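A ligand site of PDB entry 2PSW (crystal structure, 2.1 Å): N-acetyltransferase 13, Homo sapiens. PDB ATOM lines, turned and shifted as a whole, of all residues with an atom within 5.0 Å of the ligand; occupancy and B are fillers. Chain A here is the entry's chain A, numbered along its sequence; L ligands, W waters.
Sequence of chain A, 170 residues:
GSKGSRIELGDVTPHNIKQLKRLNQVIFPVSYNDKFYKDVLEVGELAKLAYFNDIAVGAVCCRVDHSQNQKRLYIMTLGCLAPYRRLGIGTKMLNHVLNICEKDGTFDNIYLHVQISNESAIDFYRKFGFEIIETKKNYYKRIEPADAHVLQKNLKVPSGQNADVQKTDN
The backbone NH of Thr 91 is in hydrogen-bond range of an oxygen (O9) of the ligand, 3.0 Å away. OG1 of Thr 91 lies within hydrogen-bond range of O9 of the ligand, 2.5 Å away. ND2 of Asn 118 lies within hydrogen-bond range of O16 of the ligand, 2.6 Å away. N of Arg 86 sits at hydrogen-bond distance from O12 of the ligand, at 2.9 Å. An oxygen (O4) of the ligand lies within salt-bridge range of the guanidinium group (NH2) of Arg 86 (2.7 Å). The backbone NH of Gly 88 lies within hydrogen-bond range of an oxygen (O8) of the ligand. An oxygen (O15) of the ligand is in hydrogen-bond range of the backbone NH (N) of Cys 80. An oxygen (O11) of the ligand is in hydrogen-bond range of the backbone NH of Gly 90 (2.8 Å). N of Leu 87 is in hydrogen-bond range of O8 of the ligand, 3.1 Å away. The side-chain amino group (NZ) of Lys 127 sits close to an oxygen (O1) of the ligand (3.4 Å). The backbone carbonyl oxygen of Leu 78 lies within hydrogen-bond range of a nitrogen (N7) of the ligand (3.3 Å). The guanidinium group of Arg 85 lies within hydrogen-bond range of an oxygen (O15) of the ligand, at 3.4 Å. The backbone NH (N) of Ile 89 is in hydrogen-bond range of an oxygen (O11) of the ligand.
The side-chain amide oxygen (OD1) of Asn 118 is in hydrogen-bond range of the backbone NH (N) of Ala 121, at 3.1 Å. The guanidinium group (NE) of Arg 85 is in hydrogen-bond range of the backbone carbonyl oxygen (O) of Cys 80.
Ile 27 touches the ligand. Phe 28 touches the ligand. Gly 79 touches the ligand. Ser 120 touches the ligand (CB to N3, 3.1 Å). Ala 121 touches the ligand (CB to C20, 3.8 Å). Asp 123 touches the ligand. CD1 of Phe 124 touches C10 of the ligand, at 3.5 Å. Hydrophobic or aromatic side chains within 4 Å of the ligand: Ile 27, Phe 28, Leu 78, Ala 121 and Phe 124. The nearest printed residue that does not touch the ligand is His 113 (4.04 Å).
Water W3 lies within hydrogen-bond range of OG of Ser 120 (2.7 Å), OD1 of Asn 118 (2.8 Å) and N6 of the ligand (2.8 Å). Water W2 bridges a sulfur (S1) of the ligand (2.9 Å) and the side-chain amide nitrogen of Asn 118 (3.1 Å).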
ATOM      1  N   ILE A  27     -12.280   4.383  12.406  1.00  0.00           N
ATOM      2  CA  ILE A  27     -11.810   4.724  11.089  1.00  0.00           C
ATOM      3  C   ILE A  27     -10.342   5.198  11.059  1.00  0.00           C
ATOM      4  O   ILE A  27      -9.597   4.841  10.139  1.00  0.00           O
ATOM      5  CB  ILE A  27     -12.746   5.817  10.495  1.00  0.00           C
ATOM      6  CG1 ILE A  27     -14.184   5.293  10.457  1.00  0.00           C
ATOM      7  CG2 ILE A  27     -12.244   6.277   9.130  1.00  0.00           C
ATOM      8  CD1 ILE A  27     -15.269   6.376  10.441  1.00  0.00           C
ATOM      9  N   PHE A  28      -9.958   6.003  12.042  1.00  0.00           N
ATOM     10  CA  PHE A  28      -8.647   6.677  12.050  1.00  0.00           C
ATOM     11  C   PHE A  28      -7.659   6.039  13.005  1.00  0.00           C
ATOM     12  O   PHE A  28      -8.020   5.699  14.138  1.00  0.00           O
ATOM     13  CB  PHE A  28      -8.817   8.170  12.343  1.00  0.00           C
ATOM     14  CG  PHE A  28      -9.699   8.856  11.347  1.00  0.00           C
ATOM     15  CD1 PHE A  28      -9.235   9.139  10.062  1.00  0.00           C
ATOM     16  CD2 PHE A  28     -11.015   9.145  11.658  1.00  0.00           C
ATOM     17  CE1 PHE A  28     -10.067   9.737   9.120  1.00  0.00           C
ATOM     18  CE2 PHE A  28     -11.867   9.739  10.723  1.00  0.00           C
ATOM     19  CZ  PHE A  28     -11.371  10.047   9.435  1.00  0.00           C
ATOM     20  N   LEU A  78     -11.520  13.032   7.785  1.00  0.00           N
ATOM     21  CA  LEU A  78     -12.638  12.850   6.856  1.00  0.00           C
ATOM     22  C   LEU A  78     -12.640  11.400   6.464  1.00  0.00           C
ATOM     23  O   LEU A  78     -11.673  10.911   5.941  1.00  0.00           O
ATOM     24  CB  LEU A  78     -12.498  13.735   5.627  1.00  0.00           C
ATOM     25  CG  LEU A  78     -13.620  13.807   4.581  1.00  0.00           C
ATOM     26  CD1 LEU A  78     -13.504  15.077   3.694  1.00  0.00           C
ATOM     27  CD2 LEU A  78     -13.542  12.575   3.702  1.00  0.00           C
ATOM     28  N   GLY A  79     -13.717  10.679   6.730  1.00  0.00           N
ATOM     29  CA  GLY A  79     -13.668   9.230   6.541  1.00  0.00           C
ATOM     30  C   GLY A  79     -14.998   8.605   6.811  1.00  0.00           C
ATOM     31  O   GLY A  79     -15.871   9.275   7.349  1.00  0.00           O
ATOM     32  N   CYS A  80     -15.190   7.375   6.346  1.00  0.00           N
ATOM     33  CA  CYS A  80     -16.323   6.539   6.746  1.00  0.00           C
ATOM     34  C   CYS A  80     -15.931   5.082   6.942  1.00  0.00           C
ATOM     35  O   CYS A  80     -14.834   4.657   6.562  1.00  0.00           O
ATOM     36  CB  CYS A  80     -17.514   6.670   5.795  1.00  0.00           C
ATOM     37  SG  CYS A  80     -17.308   5.954   4.139  1.00  0.00           S
ATOM     38  N   TYR A  84     -18.933   0.809   3.945  1.00  0.00           N
ATOM     39  CA  TYR A  84     -19.741   1.819   3.232  1.00  0.00           C
ATOM     40  C   TYR A  84     -18.900   2.679   2.231  1.00  0.00           C
ATOM     41  O   TYR A  84     -19.382   3.720   1.709  1.00  0.00           O
ATOM     42  CB  TYR A  84     -20.474   2.732   4.249  1.00  0.00           C
ATOM     43  CG  TYR A  84     -21.451   1.968   5.107  1.00  0.00           C
ATOM     44  CD1 TYR A  84     -22.728   1.714   4.674  1.00  0.00           C
ATOM     45  CD2 TYR A  84     -21.067   1.461   6.336  1.00  0.00           C
ATOM     46  CE1 TYR A  84     -23.638   0.988   5.456  1.00  0.00           C
ATOM     47  CE2 TYR A  84     -21.968   0.715   7.129  1.00  0.00           C
ATOM     48  CZ  TYR A  84     -23.234   0.480   6.686  1.00  0.00           C
ATOM     49  OH  TYR A  84     -24.112  -0.235   7.467  1.00  0.00           O
ATOM     50  N   ARG A  85     -17.668   2.253   1.963  1.00  0.00           N
ATOM     51  CA  ARG A  85     -16.810   3.054   1.130  1.00  0.00           C
ATOM     52  C   ARG A  85     -17.192   2.847  -0.354  1.00  0.00           C
ATOM     53  O   ARG A  85     -17.841   1.862  -0.682  1.00  0.00           O
ATOM     54  CB  ARG A  85     -15.340   2.767   1.413  1.00  0.00           C
ATOM     55  CG  ARG A  85     -14.876   3.384   2.726  1.00  0.00           C
ATOM     56  CD  ARG A  85     -13.449   3.089   3.059  1.00  0.00           C
ATOM     57  NE  ARG A  85     -13.260   3.361   4.482  1.00  0.00           N
ATOM     58  CZ  ARG A  85     -12.236   2.909   5.204  1.00  0.00           C
ATOM     59  NH1 ARG A  85     -11.273   2.206   4.603  1.00  0.00           N
ATOM     60  NH2 ARG A  85     -12.183   3.184   6.529  1.00  0.00           N
ATOM     61  N   ARG A  86     -16.822   3.805  -1.200  1.00  0.00           N
ATOM     62  CA  ARG A  86     -17.081   3.757  -2.658  1.00  0.00           C
ATOM     63  C   ARG A  86     -18.547   3.875  -2.911  1.00  0.00           C
ATOM     64  O   ARG A  86     -19.054   3.296  -3.859  1.00  0.00           O
ATOM     65  CB  ARG A  86     -16.524   2.498  -3.310  1.00  0.00           C
ATOM     66  CG  ARG A  86     -14.988   2.414  -3.442  1.00  0.00           C
ATOM     67  CD  ARG A  86     -14.353   3.721  -3.968  1.00  0.00           C
ATOM     68  NE  ARG A  86     -14.217   3.829  -5.434  1.00  0.00           N
ATOM     69  CZ  ARG A  86     -13.382   3.087  -6.161  1.00  0.00           C
ATOM     70  NH1 ARG A  86     -12.653   2.151  -5.565  1.00  0.00           N
ATOM     71  NH2 ARG A  86     -13.277   3.267  -7.482  1.00  0.00           N
ATOM     72  N   LEU A  87     -19.224   4.646  -2.061  1.00  0.00           N
ATOM     73  CA  LEU A  87     -20.655   4.871  -2.224  1.00  0.00           C
ATOM     74  C   LEU A  87     -20.976   6.360  -2.366  1.00  0.00           C
ATOM     75  O   LEU A  87     -22.124   6.757  -2.464  1.00  0.00           O
ATOM     76  CB  LEU A  87     -21.432   4.247  -1.075  1.00  0.00           C
ATOM     77  CG  LEU A  87     -21.571   2.726  -1.027  1.00  0.00           C
ATOM     78  CD1 LEU A  87     -22.330   2.389   0.251  1.00  0.00           C
ATOM     79  CD2 LEU A  87     -22.309   2.232  -2.271  1.00  0.00           C
ATOM     80  N   GLY A  88     -19.932   7.172  -2.412  1.00  0.00           N
ATOM     81  CA  GLY A  88     -20.098   8.595  -2.560  1.00  0.00           C
ATOM     82  C   GLY A  88     -20.127   9.330  -1.239  1.00  0.00           C
ATOM     83  O   GLY A  88     -20.369  10.538  -1.215  1.00  0.00           O
ATOM     84  N   ILE A  89     -19.842   8.656  -0.113  1.00  0.00           N
ATOM     85  CA  ILE A  89     -20.001   9.362   1.137  1.00  0.00           C
ATOM     86  C   ILE A  89     -18.843  10.321   1.291  1.00  0.00           C
ATOM     87  O   ILE A  89     -19.036  11.410   1.776  1.00  0.00           O
ATOM     88  CB  ILE A  89     -20.185   8.421   2.345  1.00  0.00           C
ATOM     89  CG1 ILE A  89     -21.478   7.630   2.172  1.00  0.00           C
ATOM     90  CG2 ILE A  89     -20.212   9.197   3.695  1.00  0.00           C
ATOM     91  CD1 ILE A  89     -21.441   6.270   2.828  1.00  0.00           C
ATOM     92  N   GLY A  90     -17.649   9.951   0.862  1.00  0.00           N
ATOM     93  CA  GLY A  90     -16.497  10.835   1.000  1.00  0.00           C
ATOM     94  C   GLY A  90     -16.716  12.107   0.202  1.00  0.00           C
ATOM     95  O   GLY A  90     -16.486  13.217   0.697  1.00  0.00           O
ATOM     96  N   THR A  91     -17.178  11.922  -1.029  1.00  0.00           N
ATOM     97  CA  THR A  91     -17.458  13.016  -1.934  1.00  0.00           C
ATOM     98  C   THR A  91     -18.456  14.017  -1.336  1.00  0.00           C
ATOM     99  O   THR A  91     -18.245  15.193  -1.386  1.00  0.00           O
ATOM    100  CB  THR A  91     -18.046  12.473  -3.257  1.00  0.00           C
ATOM    101  OG1 THR A  91     -17.090  11.572  -3.838  1.00  0.00           O
ATOM    102  CG2 THR A  91     -18.328  13.603  -4.248  1.00  0.00           C
ATOM    103  N   LEU A 112      -4.336  18.706   4.013  1.00  0.00           N
ATOM    104  CA  LEU A 112      -4.450  17.642   5.009  1.00  0.00           C
ATOM    105  C   LEU A 112      -3.193  16.775   4.948  1.00  0.00           C
ATOM    106  O   LEU A 112      -2.377  16.918   4.043  1.00  0.00           O
ATOM    107  CB  LEU A 112      -5.686  16.773   4.750  1.00  0.00           C
ATOM    108  CG  LEU A 112      -5.664  15.787   3.559  1.00  0.00           C
ATOM    109  CD1 LEU A 112      -6.361  14.508   3.963  1.00  0.00           C
ATOM    110  CD2 LEU A 112      -6.294  16.372   2.359  1.00  0.00           C
ATOM    111  N   HIS A 113      -3.063  15.858   5.925  1.00  0.00           N
ATOM    112  CA  HIS A 113      -1.970  14.885   5.957  1.00  0.00           C
ATOM    113  C   HIS A 113      -2.509  13.482   5.728  1.00  0.00           C
ATOM    114  O   HIS A 113      -3.514  13.073   6.329  1.00  0.00           O
ATOM    115  CB  HIS A 113      -1.212  14.944   7.278  1.00  0.00           C
ATOM    116  CG  HIS A 113      -0.452  16.212   7.473  1.00  0.00           C
ATOM    117  ND1 HIS A 113       0.855  16.369   7.069  1.00  0.00           N
ATOM    118  CD2 HIS A 113      -0.820  17.397   8.008  1.00  0.00           C
ATOM    119  CE1 HIS A 113       1.266  17.597   7.347  1.00  0.00           C
ATOM    120  NE2 HIS A 113       0.270  18.248   7.920  1.00  0.00           N
ATOM    121  N   VAL A 114      -1.826  12.757   4.849  1.00  0.00           N
ATOM    122  CA  VAL A 114      -2.147  11.383   4.528  1.00  0.00           C
ATOM    123  C   VAL A 114      -0.902  10.516   4.711  1.00  0.00           C
ATOM    124  O   VAL A 114       0.142  10.777   4.108  1.00  0.00           O
ATOM    125  CB  VAL A 114      -2.631  11.292   3.078  1.00  0.00           C
ATOM    126  CG1 VAL A 114      -2.510   9.899   2.508  1.00  0.00           C
ATOM    127  CG2 VAL A 114      -4.075  11.752   2.981  1.00  0.00           C
ATOM    128  N   ASN A 118      -1.609   5.232   2.408  1.00  0.00           N
ATOM    129  CA  ASN A 118      -3.029   5.411   2.153  1.00  0.00           C
ATOM    130  C   ASN A 118      -3.300   5.701   0.686  1.00  0.00           C
ATOM    131  O   ASN A 118      -3.682   6.817   0.313  1.00  0.00           O
ATOM    132  CB  ASN A 118      -3.572   6.578   2.987  1.00  0.00           C
ATOM    133  CG  ASN A 118      -5.055   6.435   3.297  1.00  0.00           C
ATOM    134  OD1 ASN A 118      -5.811   5.850   2.514  1.00  0.00           O
ATOM    135  ND2 ASN A 118      -5.474   6.973   4.439  1.00  0.00           N
ATOM    136  N   SER A 120      -5.702   4.726  -1.300  1.00  0.00           N
ATOM    137  CA  SER A 120      -7.068   5.044  -1.599  1.00  0.00           C
ATOM    138  C   SER A 120      -7.402   6.516  -1.265  1.00  0.00           C
ATOM    139  O   SER A 120      -8.105   7.198  -2.024  1.00  0.00           O
ATOM    140  CB  SER A 120      -7.996   4.046  -0.899  1.00  0.00           C
ATOM    141  OG  SER A 120      -8.380   4.483   0.384  1.00  0.00           O
ATOM    142  N   ALA A 121      -6.869   7.013  -0.150  1.00  0.00           N
ATOM    143  CA  ALA A 121      -7.019   8.419   0.194  1.00  0.00           C
ATOM    144  C   ALA A 121      -6.342   9.348  -0.825  1.00  0.00           C
ATOM    145  O   ALA A 121      -6.916  10.348  -1.176  1.00  0.00           O
ATOM    146  CB  ALA A 121      -6.505   8.723   1.600  1.00  0.00           C
ATOM    147  N   ASP A 123      -5.679   8.668  -4.075  1.00  0.00           N
ATOM    148  CA  ASP A 123      -6.601   8.554  -5.218  1.00  0.00           C
ATOM    149  C   ASP A 123      -7.839   9.448  -5.076  1.00  0.00           C
ATOM    150  O   ASP A 123      -8.188  10.178  -5.998  1.00  0.00           O
ATOM    151  CB  ASP A 123      -7.096   7.131  -5.335  1.00  0.00           C
ATOM    152  CG  ASP A 123      -6.278   6.291  -6.305  1.00  0.00           C
ATOM    153  OD1 ASP A 123      -5.753   6.853  -7.314  1.00  0.00           O
ATOM    154  OD2 ASP A 123      -6.230   5.058  -6.072  1.00  0.00           O
ATOM    155  N   PHE A 124      -8.513   9.342  -3.922  1.00  0.00           N
ATOM    156  CA  PHE A 124      -9.694  10.160  -3.606  1.00  0.00           C
ATOM    157  C   PHE A 124      -9.403  11.670  -3.719  1.00  0.00           C
ATOM    158  O   PHE A 124     -10.050  12.412  -4.480  1.00  0.00           O
ATOM    159  CB  PHE A 124     -10.169   9.816  -2.181  1.00  0.00           C
ATOM    160  CG  PHE A 124     -11.274  10.705  -1.661  1.00  0.00           C
ATOM    161  CD1 PHE A 124     -12.570  10.568  -2.136  1.00  0.00           C
ATOM    162  CD2 PHE A 124     -11.025  11.673  -0.724  1.00  0.00           C
ATOM    163  CE1 PHE A 124     -13.577  11.385  -1.693  1.00  0.00           C
ATOM    164  CE2 PHE A 124     -12.044  12.490  -0.245  1.00  0.00           C
ATOM    165  CZ  PHE A 124     -13.318  12.347  -0.748  1.00  0.00           C
ATOM    166  N   TYR A 125      -8.413  12.140  -2.981  1.00  0.00           N
ATOM    167  CA  TYR A 125      -8.152  13.588  -2.969  1.00  0.00           C
ATOM    168  C   TYR A 125      -7.618  14.097  -4.285  1.00  0.00           C
ATOM    169  O   TYR A 125      -7.877  15.244  -4.660  1.00  0.00           O
ATOM    170  CB  TYR A 125      -7.218  13.965  -1.836  1.00  0.00           C
ATOM    171  CG  TYR A 125      -7.938  13.990  -0.533  1.00  0.00           C
ATOM    172  CD1 TYR A 125      -8.821  15.011  -0.216  1.00  0.00           C
ATOM    173  CD2 TYR A 125      -7.753  12.973   0.391  1.00  0.00           C
ATOM    174  CE1 TYR A 125      -9.510  15.015   1.026  1.00  0.00           C
ATOM    175  CE2 TYR A 125      -8.433  12.968   1.628  1.00  0.00           C
ATOM    176  CZ  TYR A 125      -9.305  13.992   1.924  1.00  0.00           C
ATOM    177  OH  TYR A 125      -9.972  13.992   3.117  1.00  0.00           O
ATOM    178  N   LYS A 127      -8.437  13.130  -7.264  1.00  0.00           N
ATOM    179  CA  LYS A 127      -9.625  13.247  -8.090  1.00  0.00           C
ATOM    180  C   LYS A 127     -10.249  14.628  -7.972  1.00  0.00           C
ATOM    181  O   LYS A 127     -10.721  15.172  -8.951  1.00  0.00           O
ATOM    182  CB  LYS A 127     -10.607  12.135  -7.745  1.00  0.00           C
ATOM    183  CG  LYS A 127     -11.960  12.287  -8.417  1.00  0.00           C
ATOM    184  CD  LYS A 127     -12.728  10.966  -8.539  1.00  0.00           C
ATOM    185  CE  LYS A 127     -12.800  10.494 -10.017  1.00  0.00           C
ATOM    186  NZ  LYS A 127     -11.481   9.989 -10.577  1.00  0.00           N
ATOM    187  N   PHE A 128     -10.171  15.236  -6.790  1.00  0.00           N
ATOM    188  CA  PHE A 128     -10.723  16.570  -6.575  1.00  0.00           C
ATOM    189  C   PHE A 128      -9.724  17.692  -6.813  1.00  0.00           C
ATOM    190  O   PHE A 128      -9.989  18.817  -6.445  1.00  0.00           O
ATOM    191  CB  PHE A 128     -11.286  16.729  -5.162  1.00  0.00           C
ATOM    192  CG  PHE A 128     -12.532  15.892  -4.910  1.00  0.00           C
ATOM    193  CD1 PHE A 128     -13.798  16.476  -4.951  1.00  0.00           C
ATOM    194  CD2 PHE A 128     -12.427  14.532  -4.639  1.00  0.00           C
ATOM    195  CE1 PHE A 128     -14.937  15.704  -4.728  1.00  0.00           C
ATOM    196  CE2 PHE A 128     -13.578  13.746  -4.414  1.00  0.00           C
ATOM    197  CZ  PHE A 128     -14.813  14.328  -4.453  1.00  0.00           C
HETATM  198  N1  LIG L   1      -9.236   3.043  -4.855  1.00  0.00           N
HETATM  199  C1  LIG L   1      -9.230   3.814  -6.017  1.00  0.00           C
HETATM  200  N2  LIG L   1      -9.951   5.008  -6.077  1.00  0.00           N
HETATM  201  C2  LIG L   1     -10.658   5.424  -5.001  1.00  0.00           C
HETATM  202  C3  LIG L   1     -10.685   4.665  -3.820  1.00  0.00           C
HETATM  203  C4  LIG L   1      -9.965   3.458  -3.758  1.00  0.00           C
HETATM  204  N3  LIG L   1     -10.039   2.651  -2.713  1.00  0.00           N
HETATM  205  N4  LIG L   1     -11.475   5.316  -2.932  1.00  0.00           N
HETATM  206  C5  LIG L   1     -11.935   6.450  -3.533  1.00  0.00           C
HETATM  207  N5  LIG L   1     -11.438   6.544  -4.813  1.00  0.00           N
HETATM  208  C6  LIG L   1     -11.694   7.619  -5.814  1.00  0.00           C
HETATM  209  C7  LIG L   1     -12.600   7.115  -6.910  1.00  0.00           C
HETATM  210  O1  LIG L   1     -12.387   7.807  -8.131  1.00  0.00           O
HETATM  211  C8  LIG L   1     -13.973   7.448  -6.379  1.00  0.00           C
HETATM  212  O2  LIG L   1     -14.905   7.513  -7.410  1.00  0.00           O
HETATM  213  P1  LIG L   1     -15.538   6.137  -7.949  1.00  0.00           P
HETATM  214  O3  LIG L   1     -16.600   6.590  -8.931  1.00  0.00           O
HETATM  215  O4  LIG L   1     -14.415   5.368  -8.641  1.00  0.00           O
HETATM  216  O5  LIG L   1     -16.179   5.303  -6.860  1.00  0.00           O
HETATM  217  C9  LIG L   1     -13.763   8.773  -5.686  1.00  0.00           C
HETATM  218  O6  LIG L   1     -12.449   8.656  -5.215  1.00  0.00           O
HETATM  219  C10 LIG L   1     -14.641   9.027  -4.472  1.00  0.00           C
HETATM  220  O7  LIG L   1     -15.225   7.872  -3.920  1.00  0.00           O
HETATM  221  P2  LIG L   1     -16.157   8.011  -2.609  1.00  0.00           P
HETATM  222  O8  LIG L   1     -17.150   6.913  -2.647  1.00  0.00           O
HETATM  223  O9  LIG L   1     -16.835   9.370  -2.646  1.00  0.00           O
HETATM  224  O10 LIG L   1     -15.124   7.927  -1.384  1.00  0.00           O
HETATM  225  P3  LIG L   1     -15.356   7.115   0.008  1.00  0.00           P
HETATM  226  O11 LIG L   1     -16.813   7.293   0.349  1.00  0.00           O
HETATM  227  O12 LIG L   1     -14.902   5.689  -0.208  1.00  0.00           O
HETATM  228  O13 LIG L   1     -14.300   7.942   0.844  1.00  0.00           O
HETATM  229  C11 LIG L   1     -12.089   7.906   1.845  1.00  0.00           C
HETATM  230  C12 LIG L   1     -12.909   7.955   0.532  1.00  0.00           C
HETATM  231  C13 LIG L   1     -10.606   8.059   1.555  1.00  0.00           C
HETATM  232  C14 LIG L   1     -12.559   9.103   2.683  1.00  0.00           C
HETATM  233  C15 LIG L   1     -12.254   6.532   2.519  1.00  0.00           C
HETATM  234  O14 LIG L   1     -11.514   5.528   1.857  1.00  0.00           O
HETATM  235  C16 LIG L   1     -11.879   6.510   3.964  1.00  0.00           C
HETATM  236  O15 LIG L   1     -12.861   6.709   4.933  1.00  0.00           O
HETATM  237  N6  LIG L   1     -10.628   6.268   4.268  1.00  0.00           N
HETATM  238  C17 LIG L   1     -10.228   6.023   5.645  1.00  0.00           C
HETATM  239  C18 LIG L   1      -9.933   7.318   6.374  1.00  0.00           C
HETATM  240  C19 LIG L   1      -8.751   8.015   5.735  1.00  0.00           C
HETATM  241  O16 LIG L   1      -7.630   7.499   5.760  1.00  0.00           O
HETATM  242  N7  LIG L   1      -8.958   9.197   5.169  1.00  0.00           N
HETATM  243  C20 LIG L   1      -7.910  10.160   4.874  1.00  0.00           C
HETATM  244  C21 LIG L   1      -7.380  11.012   6.041  1.00  0.00           C
HETATM  245  S1  LIG L   1      -6.233  10.216   7.207  1.00  0.00           S
HETATM  246  O   HOH W   1     -12.702   4.535  -0.555  1.00  0.00           O
HETATM  247  O   HOH W   2      -3.932   8.659   6.539  1.00  0.00           O
HETATM  248  O   HOH W   3      -8.416   5.113   3.002  1.00  0.00           O
HETATM  249  O   HOH W   4     -18.014   6.533  -5.552  1.00  0.00           O
